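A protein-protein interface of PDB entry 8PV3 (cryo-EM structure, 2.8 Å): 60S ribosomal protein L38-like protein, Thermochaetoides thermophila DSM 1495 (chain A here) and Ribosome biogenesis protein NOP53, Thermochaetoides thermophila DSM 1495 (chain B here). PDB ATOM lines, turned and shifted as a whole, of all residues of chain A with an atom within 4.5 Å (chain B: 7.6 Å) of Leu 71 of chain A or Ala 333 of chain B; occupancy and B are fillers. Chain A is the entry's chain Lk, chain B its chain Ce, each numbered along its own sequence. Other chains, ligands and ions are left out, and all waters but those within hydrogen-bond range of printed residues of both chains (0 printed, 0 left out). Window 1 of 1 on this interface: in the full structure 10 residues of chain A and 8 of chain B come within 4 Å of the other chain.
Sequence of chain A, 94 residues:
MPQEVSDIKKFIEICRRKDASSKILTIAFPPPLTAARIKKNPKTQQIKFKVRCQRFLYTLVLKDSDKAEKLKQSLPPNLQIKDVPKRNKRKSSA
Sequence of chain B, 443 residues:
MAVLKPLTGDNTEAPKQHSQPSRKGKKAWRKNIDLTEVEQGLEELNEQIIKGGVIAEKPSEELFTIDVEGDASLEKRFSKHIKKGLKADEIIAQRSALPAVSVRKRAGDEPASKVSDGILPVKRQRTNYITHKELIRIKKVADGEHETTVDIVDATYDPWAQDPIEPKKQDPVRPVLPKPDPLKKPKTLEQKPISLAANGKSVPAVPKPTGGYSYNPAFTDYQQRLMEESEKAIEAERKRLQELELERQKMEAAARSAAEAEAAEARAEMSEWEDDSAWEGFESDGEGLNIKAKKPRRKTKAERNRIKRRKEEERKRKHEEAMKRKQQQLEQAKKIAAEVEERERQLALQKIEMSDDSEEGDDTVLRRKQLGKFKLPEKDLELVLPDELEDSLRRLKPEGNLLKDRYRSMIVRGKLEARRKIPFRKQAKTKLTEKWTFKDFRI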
ATOM      1  N   ILE A   8      -0.549  20.653  13.598  1.00  0.00           N
ATOM      2  CA  ILE A   8       0.664  20.097  14.190  1.00  0.00           C
ATOM      3  C   ILE A   8       1.782  21.131  14.182  1.00  0.00           C
ATOM      4  O   ILE A   8       2.571  21.217  15.129  1.00  0.00           O
ATOM      5  CB  ILE A   8       1.076  18.809  13.452  1.00  0.00           C
ATOM      6  CG1 ILE A   8      -0.131  17.889  13.274  1.00  0.00           C
ATOM      7  CG2 ILE A   8       2.183  18.090  14.207  1.00  0.00           C
ATOM      8  CD1 ILE A   8      -0.685  17.352  14.572  1.00  0.00           C
ATOM      9  N   PHE A  49      -2.280  15.634  23.663  1.00  0.00           N
ATOM     10  CA  PHE A  49      -1.077  16.367  24.028  1.00  0.00           C
ATOM     11  C   PHE A  49      -1.513  17.688  24.644  1.00  0.00           C
ATOM     12  O   PHE A  49      -2.094  18.525  23.950  1.00  0.00           O
ATOM     13  CB  PHE A  49      -0.227  16.635  22.788  1.00  0.00           C
ATOM     14  CG  PHE A  49       0.424  15.420  22.205  1.00  0.00           C
ATOM     15  CD1 PHE A  49      -0.253  14.621  21.301  1.00  0.00           C
ATOM     16  CD2 PHE A  49       1.754  15.151  22.464  1.00  0.00           C
ATOM     17  CE1 PHE A  49       0.357  13.515  20.746  1.00  0.00           C
ATOM     18  CE2 PHE A  49       2.373  14.052  21.905  1.00  0.00           C
ATOM     19  CZ  PHE A  49       1.674  13.235  21.046  1.00  0.00           C
ATOM     20  N   LEU A  60      -3.921  19.136  21.827  1.00  0.00           N
ATOM     21  CA  LEU A  60      -3.942  18.522  20.507  1.00  0.00           C
ATOM     22  C   LEU A  60      -4.526  17.123  20.648  1.00  0.00           C
ATOM     23  O   LEU A  60      -4.061  16.338  21.481  1.00  0.00           O
ATOM     24  CB  LEU A  60      -2.537  18.467  19.910  1.00  0.00           C
ATOM     25  CG  LEU A  60      -2.327  17.621  18.656  1.00  0.00           C
ATOM     26  CD1 LEU A  60      -3.022  18.240  17.460  1.00  0.00           C
ATOM     27  CD2 LEU A  60      -0.844  17.443  18.386  1.00  0.00           C
ATOM     28  N   LEU A  62      -5.334  13.530  18.872  1.00  0.00           N
ATOM     29  CA  LEU A  62      -4.923  12.659  17.784  1.00  0.00           C
ATOM     30  C   LEU A  62      -5.456  11.256  18.031  1.00  0.00           C
ATOM     31  O   LEU A  62      -5.906  10.927  19.130  1.00  0.00           O
ATOM     32  CB  LEU A  62      -3.398  12.612  17.642  1.00  0.00           C
ATOM     33  CG  LEU A  62      -2.691  13.916  17.278  1.00  0.00           C
ATOM     34  CD1 LEU A  62      -1.201  13.769  17.481  1.00  0.00           C
ATOM     35  CD2 LEU A  62      -3.002  14.307  15.847  1.00  0.00           C
ATOM     36  N   LYS A  67       2.616   6.864  15.152  1.00  0.00           N
ATOM     37  CA  LYS A  67       3.015   8.218  14.778  1.00  0.00           C
ATOM     38  C   LYS A  67       2.702   9.207  15.896  1.00  0.00           C
ATOM     39  O   LYS A  67       3.482  10.134  16.162  1.00  0.00           O
ATOM     40  CB  LYS A  67       2.312   8.627  13.485  1.00  0.00           C
ATOM     41  CG  LYS A  67       2.409   7.591  12.373  1.00  0.00           C
ATOM     42  CD  LYS A  67       3.847   7.323  11.964  1.00  0.00           C
ATOM     43  CE  LYS A  67       4.495   8.557  11.362  1.00  0.00           C
ATOM     44  NZ  LYS A  67       5.894   8.292  10.928  1.00  0.00           N
ATOM     45  N   ALA A  68       1.561   9.018  16.564  1.00  0.00           N
ATOM     46  CA  ALA A  68       1.211   9.849  17.710  1.00  0.00           C
ATOM     47  C   ALA A  68       2.207   9.661  18.846  1.00  0.00           C
ATOM     48  O   ALA A  68       2.580  10.622  19.526  1.00  0.00           O
ATOM     49  CB  ALA A  68      -0.208   9.529  18.175  1.00  0.00           C
ATOM     50  N   GLU A  69       2.650   8.421  19.070  1.00  0.00           N
ATOM     51  CA  GLU A  69       3.683   8.192  20.078  1.00  0.00           C
ATOM     52  C   GLU A  69       5.027   8.771  19.643  1.00  0.00           C
ATOM     53  O   GLU A  69       5.829   9.198  20.482  1.00  0.00           O
ATOM     54  CB  GLU A  69       3.811   6.697  20.374  1.00  0.00           C
ATOM     55  CG  GLU A  69       2.505   6.017  20.761  1.00  0.00           C
ATOM     56  CD  GLU A  69       2.086   6.294  22.195  1.00  0.00           C
ATOM     57  OE1 GLU A  69       2.887   6.874  22.959  1.00  0.00           O
ATOM     58  OE2 GLU A  69       0.950   5.927  22.560  1.00  0.00           O
ATOM     59  N   LYS A  70       5.291   8.790  18.334  1.00  0.00           N
ATOM     60  CA  LYS A  70       6.554   9.301  17.813  1.00  0.00           C
ATOM     61  C   LYS A  70       6.623  10.823  17.876  1.00  0.00           C
ATOM     62  O   LYS A  70       7.727  11.377  17.919  1.00  0.00           O
ATOM     63  CB  LYS A  70       6.745   8.780  16.377  1.00  0.00           C
ATOM     64  CG  LYS A  70       8.034   9.176  15.632  1.00  0.00           C
ATOM     65  CD  LYS A  70       7.874  10.426  14.766  1.00  0.00           C
ATOM     66  CE  LYS A  70       7.001  10.152  13.557  1.00  0.00           C
ATOM     67  NZ  LYS A  70       6.845  11.356  12.696  1.00  0.00           N
ATOM     68  N   LEU A  71       5.469  11.503  17.886  1.00  0.00           N
ATOM     69  CA  LEU A  71       5.446  12.968  17.960  1.00  0.00           C
ATOM     70  C   LEU A  71       6.130  13.499  19.222  1.00  0.00           C
ATOM     71  O   LEU A  71       6.636  14.632  19.227  1.00  0.00           O
ATOM     72  CB  LEU A  71       4.000  13.465  17.885  1.00  0.00           C
ATOM     73  CG  LEU A  71       3.726  14.973  17.878  1.00  0.00           C
ATOM     74  CD1 LEU A  71       4.340  15.625  16.656  1.00  0.00           C
ATOM     75  CD2 LEU A  71       2.238  15.256  17.943  1.00  0.00           C
ATOM     76  N   LYS A  72       6.170  12.692  20.287  1.00  0.00           N
ATOM     77  CA  LYS A  72       6.904  13.059  21.495  1.00  0.00           C
ATOM     78  C   LYS A  72       8.388  13.272  21.214  1.00  0.00           C
ATOM     79  O   LYS A  72       9.012  14.155  21.814  1.00  0.00           O
ATOM     80  CB  LYS A  72       6.712  11.978  22.560  1.00  0.00           C
ATOM     81  CG  LYS A  72       7.388  12.263  23.890  1.00  0.00           C
ATOM     82  CD  LYS A  72       6.892  11.324  24.979  1.00  0.00           C
ATOM     83  CE  LYS A  72       6.957   9.871  24.537  1.00  0.00           C
ATOM     84  NZ  LYS A  72       6.439   8.950  25.585  1.00  0.00           N
ATOM     85  N   GLN A  73       8.965  12.486  20.301  1.00  0.00           N
ATOM     86  CA  GLN A  73      10.362  12.668  19.928  1.00  0.00           C
ATOM     87  C   GLN A  73      10.603  13.979  19.194  1.00  0.00           C
ATOM     88  O   GLN A  73      11.637  14.617  19.417  1.00  0.00           O
ATOM     89  CB  GLN A  73      10.834  11.497  19.064  1.00  0.00           C
ATOM     90  CG  GLN A  73      10.818  10.159  19.779  1.00  0.00           C
ATOM     91  CD  GLN A  73      11.819  10.096  20.914  1.00  0.00           C
ATOM     92  OE1 GLN A  73      12.930  10.614  20.806  1.00  0.00           O
ATOM     93  NE2 GLN A  73      11.428   9.459  22.013  1.00  0.00           N
ATOM     94  N   SER A  74       9.681  14.397  18.330  1.00  0.00           N
ATOM     95  CA  SER A  74       9.800  15.661  17.618  1.00  0.00           C
ATOM     96  C   SER A  74       9.440  16.859  18.484  1.00  0.00           C
ATOM     97  O   SER A  74       9.733  17.994  18.099  1.00  0.00           O
ATOM     98  CB  SER A  74       8.925  15.650  16.363  1.00  0.00           C
ATOM     99  OG  SER A  74       7.636  15.142  16.651  1.00  0.00           O
ATOM    100  N   LEU A  75       8.796  16.635  19.630  1.00  0.00           N
ATOM    101  CA  LEU A  75       8.651  17.724  20.587  1.00  0.00           C
ATOM    102  C   LEU A  75      10.008  18.108  21.169  1.00  0.00           C
ATOM    103  O   LEU A  75      10.939  17.297  21.176  1.00  0.00           O
ATOM    104  CB  LEU A  75       7.696  17.326  21.710  1.00  0.00           C
ATOM    105  CG  LEU A  75       6.237  17.103  21.319  1.00  0.00           C
ATOM    106  CD1 LEU A  75       5.440  16.582  22.501  1.00  0.00           C
ATOM    107  CD2 LEU A  75       5.628  18.382  20.774  1.00  0.00           C
ATOM    108  N   GLN B 327      -4.018  14.253  10.114  1.00  0.00           N
ATOM    109  CA  GLN B 327      -3.294  12.984  10.118  1.00  0.00           C
ATOM    110  C   GLN B 327      -2.058  13.038   9.226  1.00  0.00           C
ATOM    111  O   GLN B 327      -0.977  12.595   9.633  1.00  0.00           O
ATOM    112  CB  GLN B 327      -4.222  11.852   9.679  1.00  0.00           C
ATOM    113  CG  GLN B 327      -3.614  10.470   9.823  1.00  0.00           C
ATOM    114  CD  GLN B 327      -3.401  10.078  11.273  1.00  0.00           C
ATOM    115  OE1 GLN B 327      -4.181  10.452  12.149  1.00  0.00           O
ATOM    116  NE2 GLN B 327      -2.337   9.327  11.533  1.00  0.00           N
ATOM    117  N   GLN B 328      -2.193  13.599   8.020  1.00  0.00           N
ATOM    118  CA  GLN B 328      -1.056  13.682   7.104  1.00  0.00           C
ATOM    119  C   GLN B 328       0.051  14.563   7.673  1.00  0.00           C
ATOM    120  O   GLN B 328       1.242  14.246   7.544  1.00  0.00           O
ATOM    121  CB  GLN B 328      -1.506  14.195   5.735  1.00  0.00           C
ATOM    122  CG  GLN B 328      -2.482  13.281   5.007  1.00  0.00           C
ATOM    123  CD  GLN B 328      -1.848  11.978   4.551  1.00  0.00           C
ATOM    124  OE1 GLN B 328      -0.630  11.882   4.402  1.00  0.00           O
ATOM    125  NE2 GLN B 328      -2.678  10.965   4.328  1.00  0.00           N
ATOM    126  N   GLN B 329      -0.322  15.665   8.332  1.00  0.00           N
ATOM    127  CA  GLN B 329       0.688  16.464   9.023  1.00  0.00           C
ATOM    128  C   GLN B 329       1.320  15.684  10.174  1.00  0.00           C
ATOM    129  O   GLN B 329       2.495  15.896  10.503  1.00  0.00           O
ATOM    130  CB  GLN B 329       0.086  17.775   9.525  1.00  0.00           C
ATOM    131  CG  GLN B 329      -0.368  18.706   8.415  1.00  0.00           C
ATOM    132  CD  GLN B 329      -1.126  19.909   8.937  1.00  0.00           C
ATOM    133  OE1 GLN B 329      -1.436  19.994  10.124  1.00  0.00           O
ATOM    134  NE2 GLN B 329      -1.426  20.851   8.049  1.00  0.00           N
ATOM    135  N   LEU B 330       0.562  14.770  10.789  1.00  0.00           N
ATOM    136  CA  LEU B 330       1.133  13.938  11.845  1.00  0.00           C
ATOM    137  C   LEU B 330       2.210  12.995  11.307  1.00  0.00           C
ATOM    138  O   LEU B 330       3.242  12.803  11.959  1.00  0.00           O
ATOM    139  CB  LEU B 330       0.037  13.158  12.571  1.00  0.00           C
ATOM    140  CG  LEU B 330       0.499  12.223  13.690  1.00  0.00           C
ATOM    141  CD1 LEU B 330       1.245  13.001  14.760  1.00  0.00           C
ATOM    142  CD2 LEU B 330      -0.682  11.483  14.289  1.00  0.00           C
ATOM    143  N   GLU B 331       2.001  12.390  10.124  1.00  0.00           N
ATOM    144  CA  GLU B 331       3.155  11.652   9.584  1.00  0.00           C
ATOM    145  C   GLU B 331       4.268  12.575   9.098  1.00  0.00           C
ATOM    146  O   GLU B 331       5.437  12.177   9.143  1.00  0.00           O
ATOM    147  CB  GLU B 331       2.892  10.657   8.428  1.00  0.00           C
ATOM    148  CG  GLU B 331       2.072   9.387   8.695  1.00  0.00           C
ATOM    149  CD  GLU B 331       0.594   9.574   8.610  1.00  0.00           C
ATOM    150  OE1 GLU B 331       0.183  10.682   8.264  1.00  0.00           O
ATOM    151  OE2 GLU B 331      -0.155   8.616   8.893  1.00  0.00           O
ATOM    152  N   GLN B 332       3.953  13.786   8.639  1.00  0.00           N
ATOM    153  CA  GLN B 332       4.985  14.705   8.171  1.00  0.00           C
ATOM    154  C   GLN B 332       5.461  15.656   9.268  1.00  0.00           C
ATOM    155  O   GLN B 332       5.921  16.761   8.976  1.00  0.00           O
ATOM    156  CB  GLN B 332       4.492  15.494   6.959  1.00  0.00           C
ATOM    157  CG  GLN B 332       4.011  14.623   5.812  1.00  0.00           C
ATOM    158  CD  GLN B 332       5.132  13.830   5.171  1.00  0.00           C
ATOM    159  OE1 GLN B 332       6.279  14.273   5.130  1.00  0.00           O
ATOM    160  NE2 GLN B 332       4.804  12.647   4.665  1.00  0.00           N
ATOM    161  N   ALA B 333       5.355  15.232  10.531  1.00  0.00           N
ATOM    162  CA  ALA B 333       5.686  16.098  11.662  1.00  0.00           C
ATOM    163  C   ALA B 333       7.170  16.461  11.713  1.00  0.00           C
ATOM    164  O   ALA B 333       7.519  17.586  12.092  1.00  0.00           O
ATOM    165  CB  ALA B 333       5.263  15.428  12.968  1.00  0.00           C
ATOM    166  N   LYS B 334       8.058  15.519  11.374  1.00  0.00           N
ATOM    167  CA  LYS B 334       9.494  15.757  11.526  1.00  0.00           C
ATOM    168  C   LYS B 334       9.995  16.848  10.584  1.00  0.00           C
ATOM    169  O   LYS B 334      10.786  17.714  10.986  1.00  0.00           O
ATOM    170  CB  LYS B 334      10.269  14.461  11.291  1.00  0.00           C
ATOM    171  CG  LYS B 334      10.377  13.571  12.513  1.00  0.00           C
ATOM    172  CD  LYS B 334      11.153  12.306  12.194  1.00  0.00           C
ATOM    173  CE  LYS B 334      12.588  12.626  11.812  1.00  0.00           C
ATOM    174  NZ  LYS B 334      13.346  13.215  12.949  1.00  0.00           N
ATOM    175  N   LYS B 335       9.545  16.821   9.327  1.00  0.00           N
ATOM    176  CA  LYS B 335       9.891  17.878   8.383  1.00  0.00           C
ATOM    177  C   LYS B 335       9.323  19.217   8.837  1.00  0.00           C
ATOM    178  O   LYS B 335       9.952  20.266   8.656  1.00  0.00           O
ATOM    179  CB  LYS B 335       9.383  17.517   6.987  1.00  0.00           C
ATOM    180  CG  LYS B 335       9.845  18.459   5.891  1.00  0.00           C
ATOM    181  CD  LYS B 335      11.349  18.380   5.701  1.00  0.00           C
ATOM    182  CE  LYS B 335      11.767  17.016   5.177  1.00  0.00           C
ATOM    183  NZ  LYS B 335      11.222  16.759   3.816  1.00  0.00           N
ATOM    184  N   ILE B 336       8.134  19.191   9.441  1.00  0.00           N
ATOM    185  CA  ILE B 336       7.528  20.402   9.989  1.00  0.00           C
ATOM    186  C   ILE B 336       8.384  20.974  11.115  1.00  0.00           C
ATOM    187  O   ILE B 336       8.612  22.188  11.184  1.00  0.00           O
ATOM    188  CB  ILE B 336       6.091  20.104  10.454  1.00  0.00           C
ATOM    189  CG1 ILE B 336       5.178  19.886   9.247  1.00  0.00           C
ATOM    190  CG2 ILE B 336       5.566  21.206  11.335  1.00  0.00           C
ATOM    191  CD1 ILE B 336       3.793  19.409   9.611  1.00  0.00           C
ATOM    192  N   ALA B 337       8.878  20.108  12.005  1.00  0.00           N
ATOM    193  CA  ALA B 337       9.753  20.562  13.083  1.00  0.00           C
ATOM    194  C   ALA B 337      11.053  21.136  12.534  1.00  0.00           C
ATOM    195  O   ALA B 337      11.568  22.137  13.053  1.00  0.00           O
ATOM    196  CB  ALA B 337      10.040  19.414  14.049  1.00  0.00           C
ATOM    197  N   ALA B 338      11.593  20.519  11.479  1.00  0.00           N
ATOM    198  CA  ALA B 338      12.789  21.053  10.834  1.00  0.00           C
ATOM    199  C   ALA B 338      12.534  22.434  10.239  1.00  0.00           C
ATOM    200  O   ALA B 338      13.372  23.334  10.367  1.00  0.00           O
ATOM    201  CB  ALA B 338      13.278  20.088   9.756  1.00  0.00           C
ATOM    202  N   GLU B 339      11.378  22.621   9.592  1.00  0.00           N
ATOM    203  CA  GLU B 339      11.034  23.928   9.033  1.00  0.00           C
ATOM    204  C   GLU B 339      10.858  24.978  10.123  1.00  0.00           C
ATOM    205  O   GLU B 339      11.278  26.129   9.955  1.00  0.00           O
ATOM    206  CB  GLU B 339       9.765  23.830   8.188  1.00  0.00           C
ATOM    207  CG  GLU B 339       9.901  22.977   6.942  1.00  0.00           C
ATOM    208  CD  GLU B 339       8.567  22.452   6.449  1.00  0.00           C
ATOM    209  OE1 GLU B 339       7.549  22.664   7.139  1.00  0.00           O
ATOM    210  OE2 GLU B 339       8.539  21.825   5.369  1.00  0.00           O
ATOM    211  N   VAL B 340      10.229  24.603  11.241  1.00  0.00           N
ATOM    212  CA  VAL B 340      10.026  25.544  12.343  1.00  0.00           C
ATOM    213  C   VAL B 340      11.368  25.964  12.938  1.00  0.00           C
ATOM    214  O   VAL B 340      11.613  27.152  13.197  1.00  0.00           O
ATOM    215  CB  VAL B 340       9.095  24.931  13.406  1.00  0.00           C
ATOM    216  CG1 VAL B 340       9.105  25.757  14.681  1.00  0.00           C
ATOM    217  CG2 VAL B 340       7.676  24.825  12.867  1.00  0.00           C
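Printed residues of chain A that touch a printed residue of chain B: Ile 8, Leu 62, Lys 67, Lys 70 and Leu 71. Among the printed residues, no Asp or Glu carboxylate lies within 4 Å of a Lys or Arg side-chain nitrogen of the other chain.
The side-chain amide nitrogen of Gln 327 of chain B is in hydrogen-bond range of the side-chain carboxylate of Glu 331 of chain B (3.5 Å). O of Leu 71 of chain A lies within hydrogen-bond range of OG of Ser 74 of chain A, at 2.8 Å.
Of the printed residues of chain B, Lys 67 of chain A touches Leu 330 (3.9 Å) and Glu 331 (3.7 Å). Ala 68 of chain A touches none of the printed residues of chain B. Of chain B, only Ala 333 (3.8 Å) comes within 4 Å of Leu 71 of chain A. Gln 73 of chain A touches none of the printed residues of chain B. Printed residues of chain A within 4 Å of Glu 331 of chain B: Lys 67 and Lys 70. Of chain A, only Leu 71 (3.8 Å) comes within 4 Å of Ala 333 of chain B. The nearest residue of chain A that does not touch Ala 333 of chain B is Ile 8 of chain A (4.3 Å).
Among the printed residues, merely in contact across the chains: Ile 8 of chain A with Gln 329 of chain B, Lys 67 of chain A with Glu 331 of chain B, Leu 62 of chain A with Leu 330 of chain B, Leu 71 of chain A with Ala 333 of chain B, Lys 67 of chain A with Leu 330 of chain B, Lys 70 of chain A with Glu 331 of chain B and Lys 70 of chain A with Leu 330 of chain B.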
